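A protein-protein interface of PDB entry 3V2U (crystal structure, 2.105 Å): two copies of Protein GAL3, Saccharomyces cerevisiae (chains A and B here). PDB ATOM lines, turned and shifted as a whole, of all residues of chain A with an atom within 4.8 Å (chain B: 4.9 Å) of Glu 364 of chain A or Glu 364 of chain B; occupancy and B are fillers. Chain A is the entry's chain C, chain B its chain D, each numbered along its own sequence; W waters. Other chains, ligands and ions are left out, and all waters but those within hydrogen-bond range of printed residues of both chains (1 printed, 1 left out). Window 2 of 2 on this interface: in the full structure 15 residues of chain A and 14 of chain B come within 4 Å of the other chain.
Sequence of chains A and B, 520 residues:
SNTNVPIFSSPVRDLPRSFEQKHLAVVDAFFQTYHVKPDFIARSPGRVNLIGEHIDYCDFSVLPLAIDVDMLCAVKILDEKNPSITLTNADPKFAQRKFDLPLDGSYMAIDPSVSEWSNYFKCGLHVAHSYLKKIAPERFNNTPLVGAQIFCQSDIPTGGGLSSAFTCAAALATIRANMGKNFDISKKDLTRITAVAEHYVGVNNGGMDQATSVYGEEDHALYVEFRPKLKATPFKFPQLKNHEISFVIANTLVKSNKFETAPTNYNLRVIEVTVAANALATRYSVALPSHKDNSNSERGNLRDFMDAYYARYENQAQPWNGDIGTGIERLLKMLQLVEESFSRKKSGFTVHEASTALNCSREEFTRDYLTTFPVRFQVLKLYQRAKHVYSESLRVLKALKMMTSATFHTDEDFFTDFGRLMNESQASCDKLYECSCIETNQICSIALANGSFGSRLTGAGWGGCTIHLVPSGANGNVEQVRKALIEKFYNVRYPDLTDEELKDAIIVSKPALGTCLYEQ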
ATOM      1  N   ASN A 359       8.127 -22.710 -14.082  1.00  0.00           N
ATOM      2  CA  ASN A 359       7.574 -22.512 -12.745  1.00  0.00           C
ATOM      3  C   ASN A 359       8.566 -22.710 -11.587  1.00  0.00           C
ATOM      4  O   ASN A 359       8.265 -23.373 -10.596  1.00  0.00           O
ATOM      5  CB  ASN A 359       6.337 -23.394 -12.525  1.00  0.00           C
ATOM      6  CG  ASN A 359       5.487 -22.903 -11.364  1.00  0.00           C
ATOM      7  OD1 ASN A 359       5.538 -21.725 -11.003  1.00  0.00           O
ATOM      8  ND2 ASN A 359       4.710 -23.801 -10.770  1.00  0.00           N
ATOM      9  N   CYS A 360       9.746 -22.123 -11.702  1.00  0.00           N
ATOM     10  CA  CYS A 360      10.718 -22.193 -10.614  1.00  0.00           C
ATOM     11  C   CYS A 360      11.451 -20.861 -10.491  1.00  0.00           C
ATOM     12  O   CYS A 360      11.269 -19.972 -11.320  1.00  0.00           O
ATOM     13  CB  CYS A 360      11.719 -23.335 -10.867  1.00  0.00           C
ATOM     14  SG  CYS A 360      12.763 -23.130 -12.341  1.00  0.00           S
ATOM     15  N   SER A 361      12.281 -20.729  -9.461  1.00  0.00           N
ATOM     16  CA  SER A 361      13.100 -19.545  -9.294  1.00  0.00           C
ATOM     17  C   SER A 361      14.260 -19.528 -10.283  1.00  0.00           C
ATOM     18  O   SER A 361      14.627 -20.570 -10.868  1.00  0.00           O
ATOM     19  CB  SER A 361      13.647 -19.476  -7.860  1.00  0.00           C
ATOM     20  OG  SER A 361      14.503 -20.580  -7.578  1.00  0.00           O
ATOM     21  N   ARG A 362      14.840 -18.344 -10.471  1.00  0.00           N
ATOM     22  CA  ARG A 362      16.049 -18.208 -11.289  1.00  0.00           C
ATOM     23  C   ARG A 362      17.157 -19.101 -10.712  1.00  0.00           C
ATOM     24  O   ARG A 362      17.899 -19.760 -11.445  1.00  0.00           O
ATOM     25  CB  ARG A 362      16.542 -16.745 -11.330  1.00  0.00           C
ATOM     26  CG  ARG A 362      17.824 -16.576 -12.195  1.00  0.00           C
ATOM     27  CD  ARG A 362      18.649 -15.338 -11.846  1.00  0.00           C
ATOM     28  NE  ARG A 362      19.020 -15.304 -10.431  1.00  0.00           N
ATOM     29  CZ  ARG A 362      20.064 -15.937  -9.903  1.00  0.00           C
ATOM     30  NH1 ARG A 362      20.876 -16.667 -10.669  1.00  0.00           N
ATOM     31  NH2 ARG A 362      20.298 -15.837  -8.598  1.00  0.00           N
ATOM     32  N   GLU A 363      17.276 -19.098  -9.393  1.00  0.00           N
ATOM     33  CA  GLU A 363      18.320 -19.859  -8.704  1.00  0.00           C
ATOM     34  C   GLU A 363      18.186 -21.361  -8.993  1.00  0.00           C
ATOM     35  O   GLU A 363      19.170 -22.043  -9.261  1.00  0.00           O
ATOM     36  CB  GLU A 363      18.261 -19.605  -7.197  1.00  0.00           C
ATOM     37  CG  GLU A 363      18.739 -18.220  -6.761  1.00  0.00           C
ATOM     38  CD  GLU A 363      17.640 -17.137  -6.794  1.00  0.00           C
ATOM     39  OE1 GLU A 363      16.492 -17.401  -7.225  1.00  0.00           O
ATOM     40  OE2 GLU A 363      17.936 -15.997  -6.379  1.00  0.00           O
ATOM     41  N   GLU A 364      16.965 -21.876  -8.943  1.00  0.00           N
ATOM     42  CA  GLU A 364      16.762 -23.302  -9.155  1.00  0.00           C
ATOM     43  C   GLU A 364      16.950 -23.648 -10.642  1.00  0.00           C
ATOM     44  O   GLU A 364      17.497 -24.701 -10.982  1.00  0.00           O
ATOM     45  CB  GLU A 364      15.377 -23.728  -8.680  1.00  0.00           C
ATOM     46  CG  GLU A 364      15.155 -25.238  -8.640  1.00  0.00           C
ATOM     47  CD  GLU A 364      15.892 -25.944  -7.476  1.00  0.00           C
ATOM     48  OE1 GLU A 364      16.839 -25.370  -6.892  1.00  0.00           O
ATOM     49  OE2 GLU A 364      15.522 -27.090  -7.152  1.00  0.00           O
ATOM     50  N   PHE A 365      16.508 -22.745 -11.509  1.00  0.00           N
ATOM     51  CA  PHE A 365      16.701 -22.905 -12.936  1.00  0.00           C
ATOM     52  C   PHE A 365      18.185 -22.988 -13.237  1.00  0.00           C
ATOM     53  O   PHE A 365      18.628 -23.845 -13.995  1.00  0.00           O
ATOM     54  CB  PHE A 365      16.083 -21.742 -13.722  1.00  0.00           C
ATOM     55  CG  PHE A 365      16.332 -21.833 -15.198  1.00  0.00           C
ATOM     56  CD1 PHE A 365      15.515 -22.615 -16.002  1.00  0.00           C
ATOM     57  CD2 PHE A 365      17.395 -21.168 -15.778  1.00  0.00           C
ATOM     58  CE1 PHE A 365      15.741 -22.711 -17.375  1.00  0.00           C
ATOM     59  CE2 PHE A 365      17.634 -21.255 -17.158  1.00  0.00           C
ATOM     60  CZ  PHE A 365      16.815 -22.034 -17.952  1.00  0.00           C
ATOM     61  N   THR A 366      18.943 -22.084 -12.629  1.00  0.00           N
ATOM     62  CA  THR A 366      20.385 -22.034 -12.802  1.00  0.00           C
ATOM     63  C   THR A 366      21.024 -23.335 -12.334  1.00  0.00           C
ATOM     64  O   THR A 366      21.805 -23.947 -13.066  1.00  0.00           O
ATOM     65  CB  THR A 366      20.989 -20.815 -12.056  1.00  0.00           C
ATOM     66  OG1 THR A 366      20.517 -19.606 -12.665  1.00  0.00           O
ATOM     67  CG2 THR A 366      22.503 -20.839 -12.107  1.00  0.00           C
ATOM     68  N   ARG A 367      20.695 -23.767 -11.121  1.00  0.00           N
ATOM     69  CA  ARG A 367      21.227 -25.024 -10.594  1.00  0.00           C
ATOM     70  C   ARG A 367      20.882 -26.226 -11.481  1.00  0.00           C
ATOM     71  O   ARG A 367      21.697 -27.123 -11.672  1.00  0.00           O
ATOM     72  CB  ARG A 367      20.707 -25.287  -9.178  1.00  0.00           C
ATOM     73  CG  ARG A 367      21.469 -24.587  -8.071  1.00  0.00           C
ATOM     74  CD  ARG A 367      20.857 -24.914  -6.715  1.00  0.00           C
ATOM     75  NE  ARG A 367      19.508 -24.369  -6.605  1.00  0.00           N
ATOM     76  CZ  ARG A 367      19.153 -23.411  -5.754  1.00  0.00           C
ATOM     77  NH1 ARG A 367      20.052 -22.908  -4.910  1.00  0.00           N
ATOM     78  NH2 ARG A 367      17.900 -22.973  -5.736  1.00  0.00           N
ATOM     79  N   ASP A 368      19.664 -26.248 -12.013  1.00  0.00           N
ATOM     80  CA  ASP A 368      19.156 -27.407 -12.745  1.00  0.00           C
ATOM     81  C   ASP A 368      19.566 -27.506 -14.219  1.00  0.00           C
ATOM     82  O   ASP A 368      19.590 -28.599 -14.764  1.00  0.00           O
ATOM     83  CB  ASP A 368      17.625 -27.467 -12.671  1.00  0.00           C
ATOM     84  CG  ASP A 368      17.128 -27.942 -11.322  1.00  0.00           C
ATOM     85  OD1 ASP A 368      17.967 -28.439 -10.539  1.00  0.00           O
ATOM     86  OD2 ASP A 368      15.906 -27.830 -11.054  1.00  0.00           O
ATOM     87  N   CYS B 360      14.243 -31.547  -5.694  1.00  0.00           N
ATOM     88  CA  CYS B 360      14.663 -30.143  -5.792  1.00  0.00           C
ATOM     89  C   CYS B 360      15.664 -29.810  -4.684  1.00  0.00           C
ATOM     90  O   CYS B 360      15.890 -30.624  -3.789  1.00  0.00           O
ATOM     91  CB  CYS B 360      13.424 -29.224  -5.706  1.00  0.00           C
ATOM     92  SG  CYS B 360      12.540 -29.236  -4.084  1.00  0.00           S
ATOM     93  N   SER B 361      16.258 -28.617  -4.726  1.00  0.00           N
ATOM     94  CA  SER B 361      17.155 -28.194  -3.656  1.00  0.00           C
ATOM     95  C   SER B 361      16.403 -27.829  -2.365  1.00  0.00           C
ATOM     96  O   SER B 361      15.186 -27.578  -2.367  1.00  0.00           O
ATOM     97  CB  SER B 361      18.007 -27.006  -4.093  1.00  0.00           C
ATOM     98  OG  SER B 361      17.206 -25.842  -4.235  1.00  0.00           O
ATOM     99  N   ARG B 362      17.146 -27.795  -1.262  1.00  0.00           N
ATOM    100  CA  ARG B 362      16.597 -27.341   0.018  1.00  0.00           C
ATOM    101  C   ARG B 362      16.076 -25.909  -0.141  1.00  0.00           C
ATOM    102  O   ARG B 362      15.006 -25.562   0.374  1.00  0.00           O
ATOM    103  CB  ARG B 362      17.661 -27.384   1.135  1.00  0.00           C
ATOM    104  CG  ARG B 362      17.138 -26.820   2.462  1.00  0.00           C
ATOM    105  CD  ARG B 362      18.249 -26.395   3.433  1.00  0.00           C
ATOM    106  NE  ARG B 362      19.072 -25.293   2.931  1.00  0.00           N
ATOM    107  CZ  ARG B 362      18.679 -24.021   2.843  1.00  0.00           C
ATOM    108  NH1 ARG B 362      17.449 -23.654   3.206  1.00  0.00           N
ATOM    109  NH2 ARG B 362      19.521 -23.108   2.379  1.00  0.00           N
ATOM    110  N   GLU B 363      16.840 -25.088  -0.859  1.00  0.00           N
ATOM    111  CA  GLU B 363      16.459 -23.694  -1.064  1.00  0.00           C
ATOM    112  C   GLU B 363      15.122 -23.595  -1.799  1.00  0.00           C
ATOM    113  O   GLU B 363      14.230 -22.840  -1.398  1.00  0.00           O
ATOM    114  CB  GLU B 363      17.540 -22.937  -1.833  1.00  0.00           C
ATOM    115  CG  GLU B 363      18.819 -22.701  -1.039  1.00  0.00           C
ATOM    116  CD  GLU B 363      19.826 -23.860  -1.104  1.00  0.00           C
ATOM    117  OE1 GLU B 363      19.501 -24.952  -1.627  1.00  0.00           O
ATOM    118  OE2 GLU B 363      20.960 -23.669  -0.617  1.00  0.00           O
ATOM    119  N   GLU B 364      14.971 -24.374  -2.859  1.00  0.00           N
ATOM    120  CA  GLU B 364      13.751 -24.284  -3.651  1.00  0.00           C
ATOM    121  C   GLU B 364      12.559 -24.841  -2.874  1.00  0.00           C
ATOM    122  O   GLU B 364      11.469 -24.266  -2.900  1.00  0.00           O
ATOM    123  CB  GLU B 364      13.905 -24.981  -5.010  1.00  0.00           C
ATOM    124  CG  GLU B 364      12.727 -24.737  -5.964  1.00  0.00           C
ATOM    125  CD  GLU B 364      12.757 -23.358  -6.650  1.00  0.00           C
ATOM    126  OE1 GLU B 364      13.528 -22.467  -6.220  1.00  0.00           O
ATOM    127  OE2 GLU B 364      12.010 -23.168  -7.637  1.00  0.00           O
ATOM    128  N   PHE B 365      12.775 -25.952  -2.177  1.00  0.00           N
ATOM    129  CA  PHE B 365      11.766 -26.505  -1.278  1.00  0.00           C
ATOM    130  C   PHE B 365      11.276 -25.455  -0.260  1.00  0.00           C
ATOM    131  O   PHE B 365      10.082 -25.316  -0.017  1.00  0.00           O
ATOM    132  CB  PHE B 365      12.313 -27.703  -0.504  1.00  0.00           C
ATOM    133  CG  PHE B 365      11.305 -28.320   0.434  1.00  0.00           C
ATOM    134  CD1 PHE B 365      10.345 -29.205  -0.046  1.00  0.00           C
ATOM    135  CD2 PHE B 365      11.294 -27.997   1.784  1.00  0.00           C
ATOM    136  CE1 PHE B 365       9.409 -29.775   0.805  1.00  0.00           C
ATOM    137  CE2 PHE B 365      10.356 -28.570   2.652  1.00  0.00           C
ATOM    138  CZ  PHE B 365       9.409 -29.448   2.166  1.00  0.00           C
ATOM    139  N   THR B 366      12.222 -24.748   0.344  1.00  0.00           N
ATOM    140  CA  THR B 366      11.918 -23.717   1.334  1.00  0.00           C
ATOM    141  C   THR B 366      11.054 -22.625   0.706  1.00  0.00           C
ATOM    142  O   THR B 366      10.037 -22.223   1.267  1.00  0.00           O
ATOM    143  CB  THR B 366      13.227 -23.142   1.922  1.00  0.00           C
ATOM    144  OG1 THR B 366      13.916 -24.195   2.610  1.00  0.00           O
ATOM    145  CG2 THR B 366      12.954 -21.984   2.911  1.00  0.00           C
ATOM    146  N   ARG B 367      11.454 -22.179  -0.482  1.00  0.00           N
ATOM    147  CA  ARG B 367      10.709 -21.162  -1.211  1.00  0.00           C
ATOM    148  C   ARG B 367       9.279 -21.602  -1.565  1.00  0.00           C
ATOM    149  O   ARG B 367       8.342 -20.804  -1.488  1.00  0.00           O
ATOM    150  CB  ARG B 367      11.476 -20.756  -2.476  1.00  0.00           C
ATOM    151  CG  ARG B 367      10.674 -19.938  -3.479  1.00  0.00           C
ATOM    152  CD  ARG B 367      11.469 -19.700  -4.766  1.00  0.00           C
ATOM    153  NE  ARG B 367      10.620 -19.351  -5.905  1.00  0.00           N
ATOM    154  CZ  ARG B 367      10.467 -18.117  -6.378  1.00  0.00           C
ATOM    155  NH1 ARG B 367      11.111 -17.104  -5.815  1.00  0.00           N
ATOM    156  NH2 ARG B 367       9.679 -17.898  -7.421  1.00  0.00           N
ATOM    157  N   ASP B 368       9.117 -22.865  -1.956  1.00  0.00           N
ATOM    158  CA  ASP B 368       7.843 -23.341  -2.502  1.00  0.00           C
ATOM    159  C   ASP B 368       6.848 -23.804  -1.446  1.00  0.00           C
ATOM    160  O   ASP B 368       5.649 -23.800  -1.688  1.00  0.00           O
ATOM    161  CB  ASP B 368       8.063 -24.506  -3.500  1.00  0.00           C
ATOM    162  CG  ASP B 368       8.716 -24.057  -4.797  1.00  0.00           C
ATOM    163  OD1 ASP B 368       8.787 -22.829  -5.046  1.00  0.00           O
ATOM    164  OD2 ASP B 368       9.170 -24.938  -5.565  1.00  0.00           O
ATOM    165  N   TYR B 369       7.345 -24.234  -0.292  1.00  0.00           N
ATOM    166  CA  TYR B 369       6.467 -24.826   0.712  1.00  0.00           C
ATOM    167  C   TYR B 369       6.508 -24.158   2.106  1.00  0.00           C
ATOM    168  O   TYR B 369       5.510 -24.190   2.827  1.00  0.00           O
ATOM    169  CB  TYR B 369       6.736 -26.332   0.821  1.00  0.00           C
ATOM    170  CG  TYR B 369       6.442 -27.061  -0.473  1.00  0.00           C
ATOM    171  CD1 TYR B 369       5.158 -27.532  -0.757  1.00  0.00           C
ATOM    172  CD2 TYR B 369       7.437 -27.257  -1.418  1.00  0.00           C
ATOM    173  CE1 TYR B 369       4.887 -28.182  -1.945  1.00  0.00           C
ATOM    174  CE2 TYR B 369       7.172 -27.900  -2.607  1.00  0.00           C
ATOM    175  CZ  TYR B 369       5.898 -28.360  -2.866  1.00  0.00           C
ATOM    176  OH  TYR B 369       5.650 -29.005  -4.046  1.00  0.00           O
HETATM  177  O   HOH W   1      17.853 -28.887  -7.791  1.00  0.00           O
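OG of Ser 361 of chain B lies within hydrogen-bond range of OE1 of Glu 364 of chain A.
OE1 of Glu 364 of chain B sits at hydrogen-bond distance from OG of Ser 361 of chain A (2.5 Å).
The side-chain hydroxyl (OG) of Ser 361 of chain B sits at hydrogen-bond distance from the guanidinium group (NH2) of Arg 367 of chain A (3.3 Å).
The side-chain carboxylate (OE1) of Glu 363 of chain B is in salt-bridge range of the guanidinium group (NH1) of Arg 367 of chain A, at 3.9 Å.
The side-chain carboxylate (OE2) of Glu 363 of chain B is in salt-bridge range of the guanidinium group (NH2) of Arg 362 of chain B, 3.4 Å away.
OG of Ser 361 of chain A sits at hydrogen-bond distance from N of Glu 364 of chain A (3.1 Å).
OE1 of Glu 364 of chain A lies within salt-bridge range of NE of Arg 367 of chain A (2.9 Å).
The side-chain hydroxyl (OG) of Ser 361 of chain B sits close to the backbone NH (N) of Glu 363 of chain B (3.5 Å).
The backbone NH (N) of Glu 364 of chain B sits at hydrogen-bond distance from the side-chain hydroxyl (OG) of Ser 361 of chain B (3.0 Å).
OE2 of Glu 364 of chain B touches CB of Cys 360 of chain A, at 3.2 Å.
CB of Ser 361 of chain A touches NE of Arg 367 of chain B, at 3.6 Å.
CB of Cys 360 of chain B touches OE2 of Glu 364 of chain A, at 3.3 Å.
Glu 364 of chain B touches Glu 364 of chain A (CB to CD, 3.3 Å).
Of chain B, only Cys 360 (3.3 Å), Ser 361 (2.7 Å) and Glu 364 (3.3 Å) come within 4 Å of Glu 364 of chain A.
Of the printed residues of chain A, Arg 367 of chain B touches Ser 361 (3.6 Å).
Printed residues of chain A within 4 Å of Glu 363 of chain B: Arg 367.
Printed residues of chain A within 4 Å of Cys 360 of chain B: Glu 364 (3.3 Å).
Printed residues of chain B within 4 Å of Ser 361 of chain A: Glu 364 (2.5 Å) and Arg 367 (3.6 Å).
The nearest printed residue of chain B that does not touch Glu 364 of chain A is Glu 363 of chain B (5.7 Å).
The nearest printed residue of chain A that does not touch Glu 364 of chain B is Arg 367 of chain A (4.3 Å).
The nearest printed residue of chain B that does not touch Cys 360 of chain A is Arg 367 of chain B (4.6 Å).
Of the 10 printed residues of chain B, 5 touch a printed residue of chain A.
Among the printed residues, 8 pairs touch across the chains.
Among the printed residues, Asp or Glu carboxylates within 4 Å of a Lys or Arg side-chain nitrogen of the other chain: Arg 367 of chain A with Glu 363 of chain B.
Cys 360 of chain A touches Glu 364 of chain B, and with the chains exchanged Glu 364 of chain A touches Cys 360 of chain B.
Ser 361 of chain A touches Arg 367 of chain B, and with the chains exchanged Arg 367 of chain A touches Ser 361 of chain B.
Glu 364 of chain B touches its own counterpart, Glu 364 of chain A.
Arg 367 of chain A touches Glu 363 of chain B, but with the chains exchanged Glu 363 of chain A does not touch Arg 367 of chain B (5.6 Å).
Positions printed for both chains: 360, 361, 362, 363, 364, 365, 366, 367 and 368.
Water W1 lies within hydrogen-bond range of the side-chain carboxylate of Asp 368 of chain A (2.8 Å), the side-chain carboxylate of Glu 364 of chain A (3.0 Å) and the backbone NH of Ser 361 of chain B (3.5 Å).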
